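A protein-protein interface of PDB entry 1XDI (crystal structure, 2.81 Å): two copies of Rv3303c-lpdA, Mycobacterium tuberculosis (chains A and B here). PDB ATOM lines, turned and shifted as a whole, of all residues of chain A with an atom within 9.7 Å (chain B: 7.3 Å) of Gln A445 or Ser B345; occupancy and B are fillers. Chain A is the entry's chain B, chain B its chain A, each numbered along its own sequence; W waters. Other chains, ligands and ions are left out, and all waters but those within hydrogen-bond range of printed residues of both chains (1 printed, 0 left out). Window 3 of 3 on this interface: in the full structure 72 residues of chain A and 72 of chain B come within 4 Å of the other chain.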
ATOM      1  N   ILE A 438      -5.854 -17.641   4.576  1.00  0.00           N
ATOM      2  CA  ILE A 438      -5.311 -18.699   5.386  1.00  0.00           C
ATOM      3  C   ILE A 438      -6.084 -18.786   6.696  1.00  0.00           C
ATOM      4  O   ILE A 438      -6.407 -17.785   7.320  1.00  0.00           O
ATOM      5  CB  ILE A 438      -3.887 -18.415   5.702  1.00  0.00           C
ATOM      6  CG1 ILE A 438      -3.152 -18.153   4.397  1.00  0.00           C
ATOM      7  CG2 ILE A 438      -3.290 -19.591   6.491  1.00  0.00           C
ATOM      8  CD1 ILE A 438      -1.765 -17.660   4.586  1.00  0.00           C
ATOM      9  N   THR A 439      -6.353 -19.994   7.147  1.00  0.00           N
ATOM     10  CA  THR A 439      -7.142 -20.179   8.350  1.00  0.00           C
ATOM     11  C   THR A 439      -6.301 -20.157   9.671  1.00  0.00           C
ATOM     12  O   THR A 439      -5.110 -20.444   9.666  1.00  0.00           O
ATOM     13  CB  THR A 439      -7.956 -21.483   8.152  1.00  0.00           C
ATOM     14  OG1 THR A 439      -9.185 -21.392   8.862  1.00  0.00           O
ATOM     15  CG2 THR A 439      -7.182 -22.696   8.624  1.00  0.00           C
ATOM     16  N   VAL A 440      -6.882 -19.794  10.806  1.00  0.00           N
ATOM     17  CA  VAL A 440      -6.043 -19.764  11.982  1.00  0.00           C
ATOM     18  C   VAL A 440      -5.618 -21.193  12.276  1.00  0.00           C
ATOM     19  O   VAL A 440      -4.528 -21.434  12.856  1.00  0.00           O
ATOM     20  CB  VAL A 440      -6.719 -19.095  13.185  1.00  0.00           C
ATOM     21  CG1 VAL A 440      -6.852 -17.645  12.931  1.00  0.00           C
ATOM     22  CG2 VAL A 440      -8.036 -19.703  13.453  1.00  0.00           C
ATOM     23  N   ASN A 441      -6.453 -22.149  11.840  1.00  0.00           N
ATOM     24  CA  ASN A 441      -6.101 -23.579  11.983  1.00  0.00           C
ATOM     25  C   ASN A 441      -4.752 -23.856  11.247  1.00  0.00           C
ATOM     26  O   ASN A 441      -3.836 -24.433  11.817  1.00  0.00           O
ATOM     27  CB  ASN A 441      -7.213 -24.499  11.423  1.00  0.00           C
ATOM     28  CG  ASN A 441      -8.505 -24.436  12.239  1.00  0.00           C
ATOM     29  OD1 ASN A 441      -9.213 -23.404  12.254  1.00  0.00           O
ATOM     30  ND2 ASN A 441      -8.820 -25.539  12.929  1.00  0.00           N
ATOM     31  N   GLU A 442      -4.642 -23.416   9.996  1.00  0.00           N
ATOM     32  CA  GLU A 442      -3.438 -23.580   9.174  1.00  0.00           C
ATOM     33  C   GLU A 442      -2.247 -22.871   9.802  1.00  0.00           C
ATOM     34  O   GLU A 442      -1.098 -23.357   9.812  1.00  0.00           O
ATOM     35  CB  GLU A 442      -3.665 -22.976   7.798  1.00  0.00           C
ATOM     36  CG  GLU A 442      -4.198 -23.934   6.725  1.00  0.00           C
ATOM     37  CD  GLU A 442      -5.454 -23.429   6.009  1.00  0.00           C
ATOM     38  OE1 GLU A 442      -5.480 -22.257   5.559  1.00  0.00           O
ATOM     39  OE2 GLU A 442      -6.424 -24.223   5.899  1.00  0.00           O
ATOM     40  N   LEU A 443      -2.523 -21.687  10.313  1.00  0.00           N
ATOM     41  CA  LEU A 443      -1.484 -20.922  10.930  1.00  0.00           C
ATOM     42  C   LEU A 443      -1.022 -21.661  12.200  1.00  0.00           C
ATOM     43  O   LEU A 443       0.170 -21.814  12.430  1.00  0.00           O
ATOM     44  CB  LEU A 443      -2.045 -19.540  11.225  1.00  0.00           C
ATOM     45  CG  LEU A 443      -1.027 -18.425  11.102  1.00  0.00           C
ATOM     46  CD1 LEU A 443      -0.100 -18.677   9.896  1.00  0.00           C
ATOM     47  CD2 LEU A 443      -1.759 -17.108  10.979  1.00  0.00           C
ATOM     48  N   ALA A 444      -1.970 -22.175  12.994  1.00  0.00           N
ATOM     49  CA  ALA A 444      -1.602 -22.819  14.256  1.00  0.00           C
ATOM     50  C   ALA A 444      -0.809 -24.060  14.037  1.00  0.00           C
ATOM     51  O   ALA A 444      -0.290 -24.637  14.989  1.00  0.00           O
ATOM     52  CB  ALA A 444      -2.828 -23.132  15.068  1.00  0.00           C
ATOM     53  N   GLN A 445      -0.741 -24.464  12.773  1.00  0.00           N
ATOM     54  CA  GLN A 445      -0.050 -25.664  12.361  1.00  0.00           C
ATOM     55  C   GLN A 445       1.380 -25.491  11.985  1.00  0.00           C
ATOM     56  O   GLN A 445       2.116 -26.462  11.957  1.00  0.00           O
ATOM     57  CB  GLN A 445      -0.727 -26.248  11.168  1.00  0.00           C
ATOM     58  CG  GLN A 445      -1.998 -26.860  11.506  1.00  0.00           C
ATOM     59  CD  GLN A 445      -2.177 -28.112  10.732  1.00  0.00           C
ATOM     60  OE1 GLN A 445      -1.343 -29.032  10.835  1.00  0.00           O
ATOM     61  NE2 GLN A 445      -3.248 -28.183   9.946  1.00  0.00           N
ATOM     62  N   THR A 446       1.750 -24.264  11.635  1.00  0.00           N
ATOM     63  CA  THR A 446       3.109 -23.942  11.253  1.00  0.00           C
ATOM     64  C   THR A 446       4.023 -24.035  12.461  1.00  0.00           C
ATOM     65  O   THR A 446       3.756 -23.435  13.509  1.00  0.00           O
ATOM     66  CB  THR A 446       3.154 -22.585  10.644  1.00  0.00           C
ATOM     67  OG1 THR A 446       2.056 -22.495   9.754  1.00  0.00           O
ATOM     68  CG2 THR A 446       4.402 -22.401   9.822  1.00  0.00           C
ATOM     69  N   LEU A 447       5.074 -24.833  12.308  1.00  0.00           N
ATOM     70  CA  LEU A 447       6.006 -25.057  13.371  1.00  0.00           C
ATOM     71  C   LEU A 447       6.943 -23.908  13.456  1.00  0.00           C
ATOM     72  O   LEU A 447       8.023 -23.972  12.904  1.00  0.00           O
ATOM     73  CB  LEU A 447       6.809 -26.340  13.132  1.00  0.00           C
ATOM     74  CG  LEU A 447       5.981 -27.620  13.400  1.00  0.00           C
ATOM     75  CD1 LEU A 447       6.509 -28.744  12.542  1.00  0.00           C
ATOM     76  CD2 LEU A 447       6.006 -28.017  14.880  1.00  0.00           C
ATOM     77  N   ALA A 448       6.552 -22.854  14.155  1.00  0.00           N
ATOM     78  CA  ALA A 448       7.416 -21.727  14.300  1.00  0.00           C
ATOM     79  C   ALA A 448       8.562 -22.048  15.254  1.00  0.00           C
ATOM     80  O   ALA A 448       8.426 -22.922  16.129  1.00  0.00           O
ATOM     81  CB  ALA A 448       6.665 -20.606  14.803  1.00  0.00           C
ATOM     82  N   VAL A 449       9.673 -21.331  15.073  1.00  0.00           N
ATOM     83  CA  VAL A 449      10.886 -21.398  15.892  1.00  0.00           C
ATOM     84  C   VAL A 449      10.648 -20.990  17.368  1.00  0.00           C
ATOM     85  O   VAL A 449      10.038 -19.967  17.626  1.00  0.00           O
ATOM     86  CB  VAL A 449      11.951 -20.341  15.417  1.00  0.00           C
ATOM     87  CG1 VAL A 449      13.195 -20.433  16.266  1.00  0.00           C
ATOM     88  CG2 VAL A 449      12.260 -20.477  13.987  1.00  0.00           C
ATOM     89  N   ILE A 457       2.516 -15.521  17.527  1.00  0.00           N
ATOM     90  CA  ILE A 457       1.586 -15.300  16.438  1.00  0.00           C
ATOM     91  C   ILE A 457       0.862 -16.647  16.282  1.00  0.00           C
ATOM     92  O   ILE A 457      -0.364 -16.717  16.218  1.00  0.00           O
ATOM     93  CB  ILE A 457       2.347 -14.965  15.158  1.00  0.00           C
ATOM     94  CG1 ILE A 457       2.884 -13.550  15.241  1.00  0.00           C
ATOM     95  CG2 ILE A 457       1.471 -15.104  13.958  1.00  0.00           C
ATOM     96  CD1 ILE A 457       4.180 -13.388  14.459  1.00  0.00           C
ATOM     97  N   THR A 458       1.665 -17.709  16.251  1.00  0.00           N
ATOM     98  CA  THR A 458       1.207 -19.089  16.119  1.00  0.00           C
ATOM     99  C   THR A 458       0.235 -19.479  17.235  1.00  0.00           C
ATOM    100  O   THR A 458      -0.799 -20.075  16.953  1.00  0.00           O
ATOM    101  CB  THR A 458       2.432 -19.986  16.015  1.00  0.00           C
ATOM    102  OG1 THR A 458       2.697 -20.219  14.619  1.00  0.00           O
ATOM    103  CG2 THR A 458       2.255 -21.279  16.755  1.00  0.00           C
ATOM    104  N   GLU A 459       0.510 -19.114  18.491  1.00  0.00           N
ATOM    105  CA  GLU A 459      -0.452 -19.421  19.559  1.00  0.00           C
ATOM    106  C   GLU A 459      -1.691 -18.486  19.499  1.00  0.00           C
ATOM    107  O   GLU A 459      -2.804 -18.920  19.848  1.00  0.00           O
ATOM    108  CB  GLU A 459       0.194 -19.298  20.950  1.00  0.00           C
ATOM    109  CG  GLU A 459       0.431 -20.627  21.678  1.00  0.00           C
ATOM    110  CD  GLU A 459      -0.783 -21.150  22.393  1.00  0.00           C
ATOM    111  OE1 GLU A 459      -1.585 -20.326  22.830  1.00  0.00           O
ATOM    112  OE2 GLU A 459      -0.914 -22.383  22.542  1.00  0.00           O
ATOM    113  N   ALA A 460      -1.521 -17.222  19.075  1.00  0.00           N
ATOM    114  CA  ALA A 460      -2.680 -16.311  19.047  1.00  0.00           C
ATOM    115  C   ALA A 460      -3.743 -17.005  18.212  1.00  0.00           C
ATOM    116  O   ALA A 460      -4.924 -17.126  18.613  1.00  0.00           O
ATOM    117  CB  ALA A 460      -2.316 -14.940  18.465  1.00  0.00           C
ATOM    118  N   ALA A 461      -3.294 -17.516  17.068  1.00  0.00           N
ATOM    119  CA  ALA A 461      -4.150 -18.225  16.144  1.00  0.00           C
ATOM    120  C   ALA A 461      -4.583 -19.574  16.708  1.00  0.00           C
ATOM    121  O   ALA A 461      -5.727 -19.954  16.589  1.00  0.00           O
ATOM    122  CB  ALA A 461      -3.419 -18.431  14.883  1.00  0.00           C
ATOM    123  N   ARG A 462      -3.664 -20.315  17.321  1.00  0.00           N
ATOM    124  CA  ARG A 462      -4.042 -21.607  17.881  1.00  0.00           C
ATOM    125  C   ARG A 462      -5.264 -21.387  18.785  1.00  0.00           C
ATOM    126  O   ARG A 462      -6.231 -22.170  18.747  1.00  0.00           O
ATOM    127  CB  ARG A 462      -2.879 -22.210  18.668  1.00  0.00           C
ATOM    128  CG  ARG A 462      -3.168 -23.576  19.141  1.00  0.00           C
ATOM    129  CD  ARG A 462      -1.966 -24.291  19.608  1.00  0.00           C
ATOM    130  NE  ARG A 462      -0.952 -24.443  18.571  1.00  0.00           N
ATOM    131  CZ  ARG A 462       0.093 -23.627  18.454  1.00  0.00           C
ATOM    132  NH1 ARG A 462       0.207 -22.624  19.308  1.00  0.00           N
ATOM    133  NH2 ARG A 462       1.049 -23.841  17.560  1.00  0.00           N
ATOM    134  N   ARG A 463      -5.248 -20.300  19.566  1.00  0.00           N
ATOM    135  CA  ARG A 463      -6.354 -19.987  20.472  1.00  0.00           C
ATOM    136  C   ARG A 463      -7.683 -19.616  19.894  1.00  0.00           C
ATOM    137  O   ARG A 463      -8.657 -19.691  20.610  1.00  0.00           O
ATOM    138  CB  ARG A 463      -5.950 -18.907  21.435  1.00  0.00           C
ATOM    139  CG  ARG A 463      -5.024 -19.485  22.434  1.00  0.00           C
ATOM    140  CD  ARG A 463      -4.681 -18.518  23.477  1.00  0.00           C
ATOM    141  NE  ARG A 463      -3.401 -18.880  24.055  1.00  0.00           N
ATOM    142  CZ  ARG A 463      -2.927 -18.366  25.170  1.00  0.00           C
ATOM    143  NH1 ARG A 463      -3.655 -17.479  25.821  1.00  0.00           N
ATOM    144  NH2 ARG A 463      -1.723 -18.722  25.596  1.00  0.00           N
ATOM    145  N   MET A 465      -8.909 -21.198  17.271  1.00  0.00           N
ATOM    146  CA  MET A 465      -9.443 -22.328  16.544  1.00  0.00           C
ATOM    147  C   MET A 465     -10.805 -22.719  17.042  1.00  0.00           C
ATOM    148  O   MET A 465     -11.031 -22.706  18.242  1.00  0.00           O
ATOM    149  CB  MET A 465      -8.501 -23.515  16.654  1.00  0.00           C
ATOM    150  CG  MET A 465      -7.278 -23.494  15.729  1.00  0.00           C
ATOM    151  SD  MET A 465      -6.213 -24.888  16.154  1.00  0.00           S
ATOM    152  CE  MET A 465      -6.436 -25.874  14.741  1.00  0.00           C
ATOM    153  N   ARG B 303       3.585 -40.718  14.038  1.00  0.00           N
ATOM    154  CA  ARG B 303       3.594 -39.485  13.281  1.00  0.00           C
ATOM    155  C   ARG B 303       2.404 -38.780  13.945  1.00  0.00           C
ATOM    156  O   ARG B 303       2.156 -37.569  13.756  1.00  0.00           O
ATOM    157  CB  ARG B 303       3.315 -39.810  11.818  1.00  0.00           C
ATOM    158  CG  ARG B 303       4.250 -39.188  10.782  1.00  0.00           C
ATOM    159  CD  ARG B 303       3.573 -39.394   9.416  1.00  0.00           C
ATOM    160  NE  ARG B 303       2.835 -40.684   9.396  1.00  0.00           N
ATOM    161  CZ  ARG B 303       1.606 -40.883   8.893  1.00  0.00           C
ATOM    162  NH1 ARG B 303       0.925 -39.883   8.347  1.00  0.00           N
ATOM    163  NH2 ARG B 303       1.065 -42.097   8.923  1.00  0.00           N
ATOM    164  N   VAL B 304       1.700 -39.579  14.751  1.00  0.00           N
ATOM    165  CA  VAL B 304       0.546 -39.122  15.494  1.00  0.00           C
ATOM    166  C   VAL B 304       0.842 -39.201  17.014  1.00  0.00           C
ATOM    167  O   VAL B 304      -0.024 -39.122  17.879  1.00  0.00           O
ATOM    168  CB  VAL B 304      -0.704 -39.882  14.926  1.00  0.00           C
ATOM    169  CG1 VAL B 304      -1.810 -40.146  15.945  1.00  0.00           C
ATOM    170  CG2 VAL B 304      -1.256 -39.012  13.824  1.00  0.00           C
ATOM    171  N   MET B 330       4.683 -29.542  19.260  1.00  0.00           N
ATOM    172  CA  MET B 330       3.685 -30.016  18.290  1.00  0.00           C
ATOM    173  C   MET B 330       3.461 -31.475  18.556  1.00  0.00           C
ATOM    174  O   MET B 330       2.404 -32.002  18.254  1.00  0.00           O
ATOM    175  CB  MET B 330       4.141 -29.864  16.829  1.00  0.00           C
ATOM    176  CG  MET B 330       2.980 -29.759  15.847  1.00  0.00           C
ATOM    177  SD  MET B 330       1.857 -28.372  16.256  1.00  0.00           S
ATOM    178  CE  MET B 330       0.324 -29.009  15.391  1.00  0.00           C
ATOM    179  N   ILE B 334      -0.301 -32.583  19.031  1.00  0.00           N
ATOM    180  CA  ILE B 334      -0.890 -33.579  18.142  1.00  0.00           C
ATOM    181  C   ILE B 334      -1.306 -34.834  18.911  1.00  0.00           C
ATOM    182  O   ILE B 334      -2.222 -35.495  18.491  1.00  0.00           O
ATOM    183  CB  ILE B 334       0.094 -33.914  16.987  1.00  0.00           C
ATOM    184  CG1 ILE B 334       0.208 -32.722  16.080  1.00  0.00           C
ATOM    185  CG2 ILE B 334      -0.371 -35.001  16.133  1.00  0.00           C
ATOM    186  CD1 ILE B 334       1.499 -32.686  15.430  1.00  0.00           C
ATOM    187  N   TYR B 337      -4.587 -33.960  20.373  1.00  0.00           N
ATOM    188  CA  TYR B 337      -5.605 -33.909  19.320  1.00  0.00           C
ATOM    189  C   TYR B 337      -6.063 -35.323  18.903  1.00  0.00           C
ATOM    190  O   TYR B 337      -7.259 -35.584  18.675  1.00  0.00           O
ATOM    191  CB  TYR B 337      -5.115 -33.110  18.074  1.00  0.00           C
ATOM    192  CG  TYR B 337      -4.827 -31.595  18.263  1.00  0.00           C
ATOM    193  CD1 TYR B 337      -5.575 -30.822  19.149  1.00  0.00           C
ATOM    194  CD2 TYR B 337      -3.743 -30.968  17.589  1.00  0.00           C
ATOM    195  CE1 TYR B 337      -5.250 -29.489  19.370  1.00  0.00           C
ATOM    196  CE2 TYR B 337      -3.414 -29.634  17.812  1.00  0.00           C
ATOM    197  CZ  TYR B 337      -4.170 -28.899  18.709  1.00  0.00           C
ATOM    198  OH  TYR B 337      -3.856 -27.575  18.986  1.00  0.00           O
ATOM    199  N   GLU B 342     -10.214 -35.009  17.930  1.00  0.00           N
ATOM    200  CA  GLU B 342     -10.297 -33.782  17.163  1.00  0.00           C
ATOM    201  C   GLU B 342      -9.673 -33.942  15.792  1.00  0.00           C
ATOM    202  O   GLU B 342      -9.295 -35.046  15.419  1.00  0.00           O
ATOM    203  CB  GLU B 342      -9.633 -32.669  17.927  1.00  0.00           C
ATOM    204  CG  GLU B 342     -10.610 -31.951  18.799  1.00  0.00           C
ATOM    205  CD  GLU B 342      -9.975 -30.769  19.504  1.00  0.00           C
ATOM    206  OE1 GLU B 342      -8.953 -30.223  19.020  1.00  0.00           O
ATOM    207  OE2 GLU B 342     -10.502 -30.363  20.565  1.00  0.00           O
ATOM    208  N   GLY B 343      -9.592 -32.876  15.012  1.00  0.00           N
ATOM    209  CA  GLY B 343      -8.964 -33.023  13.708  1.00  0.00           C
ATOM    210  C   GLY B 343      -7.466 -33.298  13.880  1.00  0.00           C
ATOM    211  O   GLY B 343      -6.827 -32.672  14.729  1.00  0.00           O
ATOM    212  N   VAL B 344      -6.878 -34.205  13.104  1.00  0.00           N
ATOM    213  CA  VAL B 344      -5.458 -34.491  13.284  1.00  0.00           C
ATOM    214  C   VAL B 344      -4.630 -34.462  12.016  1.00  0.00           C
ATOM    215  O   VAL B 344      -4.989 -35.109  11.064  1.00  0.00           O
ATOM    216  CB  VAL B 344      -5.209 -35.902  13.877  1.00  0.00           C
ATOM    217  CG1 VAL B 344      -3.740 -36.063  14.136  1.00  0.00           C
ATOM    218  CG2 VAL B 344      -5.972 -36.113  15.123  1.00  0.00           C
ATOM    219  N   SER B 345      -3.492 -33.777  12.041  1.00  0.00           N
ATOM    220  CA  SER B 345      -2.581 -33.722  10.901  1.00  0.00           C
ATOM    221  C   SER B 345      -1.176 -34.167  11.304  1.00  0.00           C
ATOM    222  O   SER B 345      -0.431 -33.386  11.907  1.00  0.00           O
ATOM    223  CB  SER B 345      -2.424 -32.285  10.387  1.00  0.00           C
ATOM    224  OG  SER B 345      -3.636 -31.545  10.387  1.00  0.00           O
ATOM    225  N   PRO B 346      -0.753 -35.389  10.953  1.00  0.00           N
ATOM    226  CA  PRO B 346       0.627 -35.813  11.345  1.00  0.00           C
ATOM    227  C   PRO B 346       1.748 -34.758  11.119  1.00  0.00           C
ATOM    228  O   PRO B 346       1.680 -33.976  10.170  1.00  0.00           O
ATOM    229  CB  PRO B 346       0.870 -37.062  10.502  1.00  0.00           C
ATOM    230  CG  PRO B 346      -0.573 -37.589  10.213  1.00  0.00           C
ATOM    231  CD  PRO B 346      -1.423 -36.362  10.062  1.00  0.00           C
ATOM    232  N   ILE B 347       2.776 -34.724  11.977  1.00  0.00           N
ATOM    233  CA  ILE B 347       3.879 -33.756  11.799  1.00  0.00           C
ATOM    234  C   ILE B 347       4.668 -34.214  10.536  1.00  0.00           C
ATOM    235  O   ILE B 347       4.893 -35.405  10.346  1.00  0.00           O
ATOM    236  CB  ILE B 347       4.915 -33.715  13.006  1.00  0.00           C
ATOM    237  CG1 ILE B 347       4.246 -33.823  14.366  1.00  0.00           C
ATOM    238  CG2 ILE B 347       5.571 -32.399  13.095  1.00  0.00           C
ATOM    239  CD1 ILE B 347       3.748 -35.311  14.745  1.00  0.00           C
ATOM    240  N   ARG B 348       5.057 -33.273   9.676  1.00  0.00           N
ATOM    241  CA  ARG B 348       5.851 -33.563   8.480  1.00  0.00           C
ATOM    242  C   ARG B 348       7.227 -32.977   8.801  1.00  0.00           C
ATOM    243  O   ARG B 348       7.338 -31.782   9.015  1.00  0.00           O
ATOM    244  CB  ARG B 348       5.295 -32.827   7.243  1.00  0.00           C
ATOM    245  CG  ARG B 348       4.027 -33.425   6.582  1.00  0.00           C
ATOM    246  CD  ARG B 348       2.997 -32.359   6.212  1.00  0.00           C
ATOM    247  NE  ARG B 348       3.238 -31.604   4.984  1.00  0.00           N
ATOM    248  CZ  ARG B 348       2.911 -30.310   4.836  1.00  0.00           C
ATOM    249  NH1 ARG B 348       2.357 -29.630   5.836  1.00  0.00           N
ATOM    250  NH2 ARG B 348       3.090 -29.677   3.676  1.00  0.00           N
ATOM    251  N   THR B 351       8.559 -29.527   7.355  1.00  0.00           N
ATOM    252  CA  THR B 351       7.825 -28.285   7.576  1.00  0.00           C
ATOM    253  C   THR B 351       8.432 -27.620   8.816  1.00  0.00           C
ATOM    254  O   THR B 351       8.274 -26.433   9.035  1.00  0.00           O
ATOM    255  CB  THR B 351       6.309 -28.520   7.768  1.00  0.00           C
ATOM    256  OG1 THR B 351       6.101 -29.420   8.860  1.00  0.00           O
ATOM    257  CG2 THR B 351       5.672 -29.061   6.493  1.00  0.00           C
ATOM    258  N   GLN B 435       4.309 -25.261   4.812  1.00  0.00           N
ATOM    259  CA  GLN B 435       3.209 -26.000   5.444  1.00  0.00           C
ATOM    260  C   GLN B 435       1.849 -25.779   4.738  1.00  0.00           C
ATOM    261  O   GLN B 435       0.942 -26.604   4.888  1.00  0.00           O
ATOM    262  CB  GLN B 435       3.069 -25.592   6.927  1.00  0.00           C
ATOM    263  CG  GLN B 435       1.834 -26.126   7.664  1.00  0.00           C
ATOM    264  CD  GLN B 435       2.105 -27.408   8.473  1.00  0.00           C
ATOM    265  OE1 GLN B 435       3.234 -27.884   8.527  1.00  0.00           O
ATOM    266  NE2 GLN B 435       1.063 -27.961   9.109  1.00  0.00           N
ATOM    267  N   ASN B 436       1.676 -24.713   3.956  1.00  0.00           N
ATOM    268  CA  ASN B 436       0.353 -24.528   3.355  1.00  0.00           C
ATOM    269  C   ASN B 436       0.288 -24.468   1.827  1.00  0.00           C
ATOM    270  O   ASN B 436      -0.740 -24.057   1.211  1.00  0.00           O
ATOM    271  CB  ASN B 436      -0.334 -23.305   3.994  1.00  0.00           C
ATOM    272  CG  ASN B 436      -0.636 -23.525   5.492  1.00  0.00           C
ATOM    273  OD1 ASN B 436      -1.320 -24.496   5.874  1.00  0.00           O
ATOM    274  ND2 ASN B 436      -0.108 -22.643   6.338  1.00  0.00           N
HETATM  275  O   HOH W   1      -1.711 -26.439  16.913  1.00  0.00           O
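The side-chain amide nitrogen (NE2) of Gln A445 is in hydrogen-bond range of the side-chain hydroxyl (OG) of Ser B345 (3.4 Å). NE2 of Gln B435 lies within hydrogen-bond range of OE1 of Gln A445.
The backbone NH (N) of Ile B347 sits close to the backbone carbonyl oxygen (O) of Arg B303 (3.4 Å). The backbone carbonyl oxygen (O) of Tyr B337 lies within hydrogen-bond range of the backbone NH (N) of Glu B342 (3.1 Å). NH1 of Arg B348 sits at hydrogen-bond distance from OE1 of Gln B435 (3.3 Å). The backbone carbonyl oxygen (O) of Glu A442 is in hydrogen-bond range of the side-chain hydroxyl (OG1) of Thr A446. The guanidinium group of Arg A462 sits at hydrogen-bond distance from the backbone carbonyl oxygen of Ala A444 (3.0 Å). The side-chain carboxylate of Glu A459 is in salt-bridge range of the guanidinium group of Arg A462 (3.4 Å).
Among the printed residues, merely in contact across the chains: Glu A442 with Asn B436, Leu A447 with Met B330, Leu A447 with Thr B351, Leu A447 with Ile B347 and Arg A462 with Tyr B337.
Val A440 touches none of the printed residues of chain B. Of the printed residues of chain B, Gln A445 touches Ser B345 and Gln B435. Of the printed residues of chain B, Arg A462 touches Tyr B337 (3.8 Å). No residue of chain A comes within 4 Å of Val B344. Ser B345 touches just one residue of chain A: Gln A445. Of the printed residues of chain A, Asn B436 touches Glu A442 (3.1 Å). The nearest residue of chain A that does not touch Ser B345 is Asn A441 (7.3 Å). The nearest printed residue of chain A that does not touch Thr B351 is Thr A446 (5.6 Å).
Hydrophobic or aromatic side chains of chain A that line the printed part of chain B: Leu A447. Along chain A the printed residues that touch a printed residue of chain B span positions 442 to 462. Printed residues of chain B that touch a printed residue of chain A: Met B330, Tyr B337, Ser B345, Ile B347, Thr B351, Gln B435 and Asn B436. Hydrophobic or aromatic side chains of chain B that line the printed part of chain A: Met B330, Tyr B337 and Ile B347.
No position is printed for both chains. Of the 7 pairs that touch across the chains among the printed residues, none has its exchanged pair printed and touching as well.
Water W1 lies within hydrogen-bond range of NE of Arg A462, O of Ala A444 and OH of Tyr B337.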
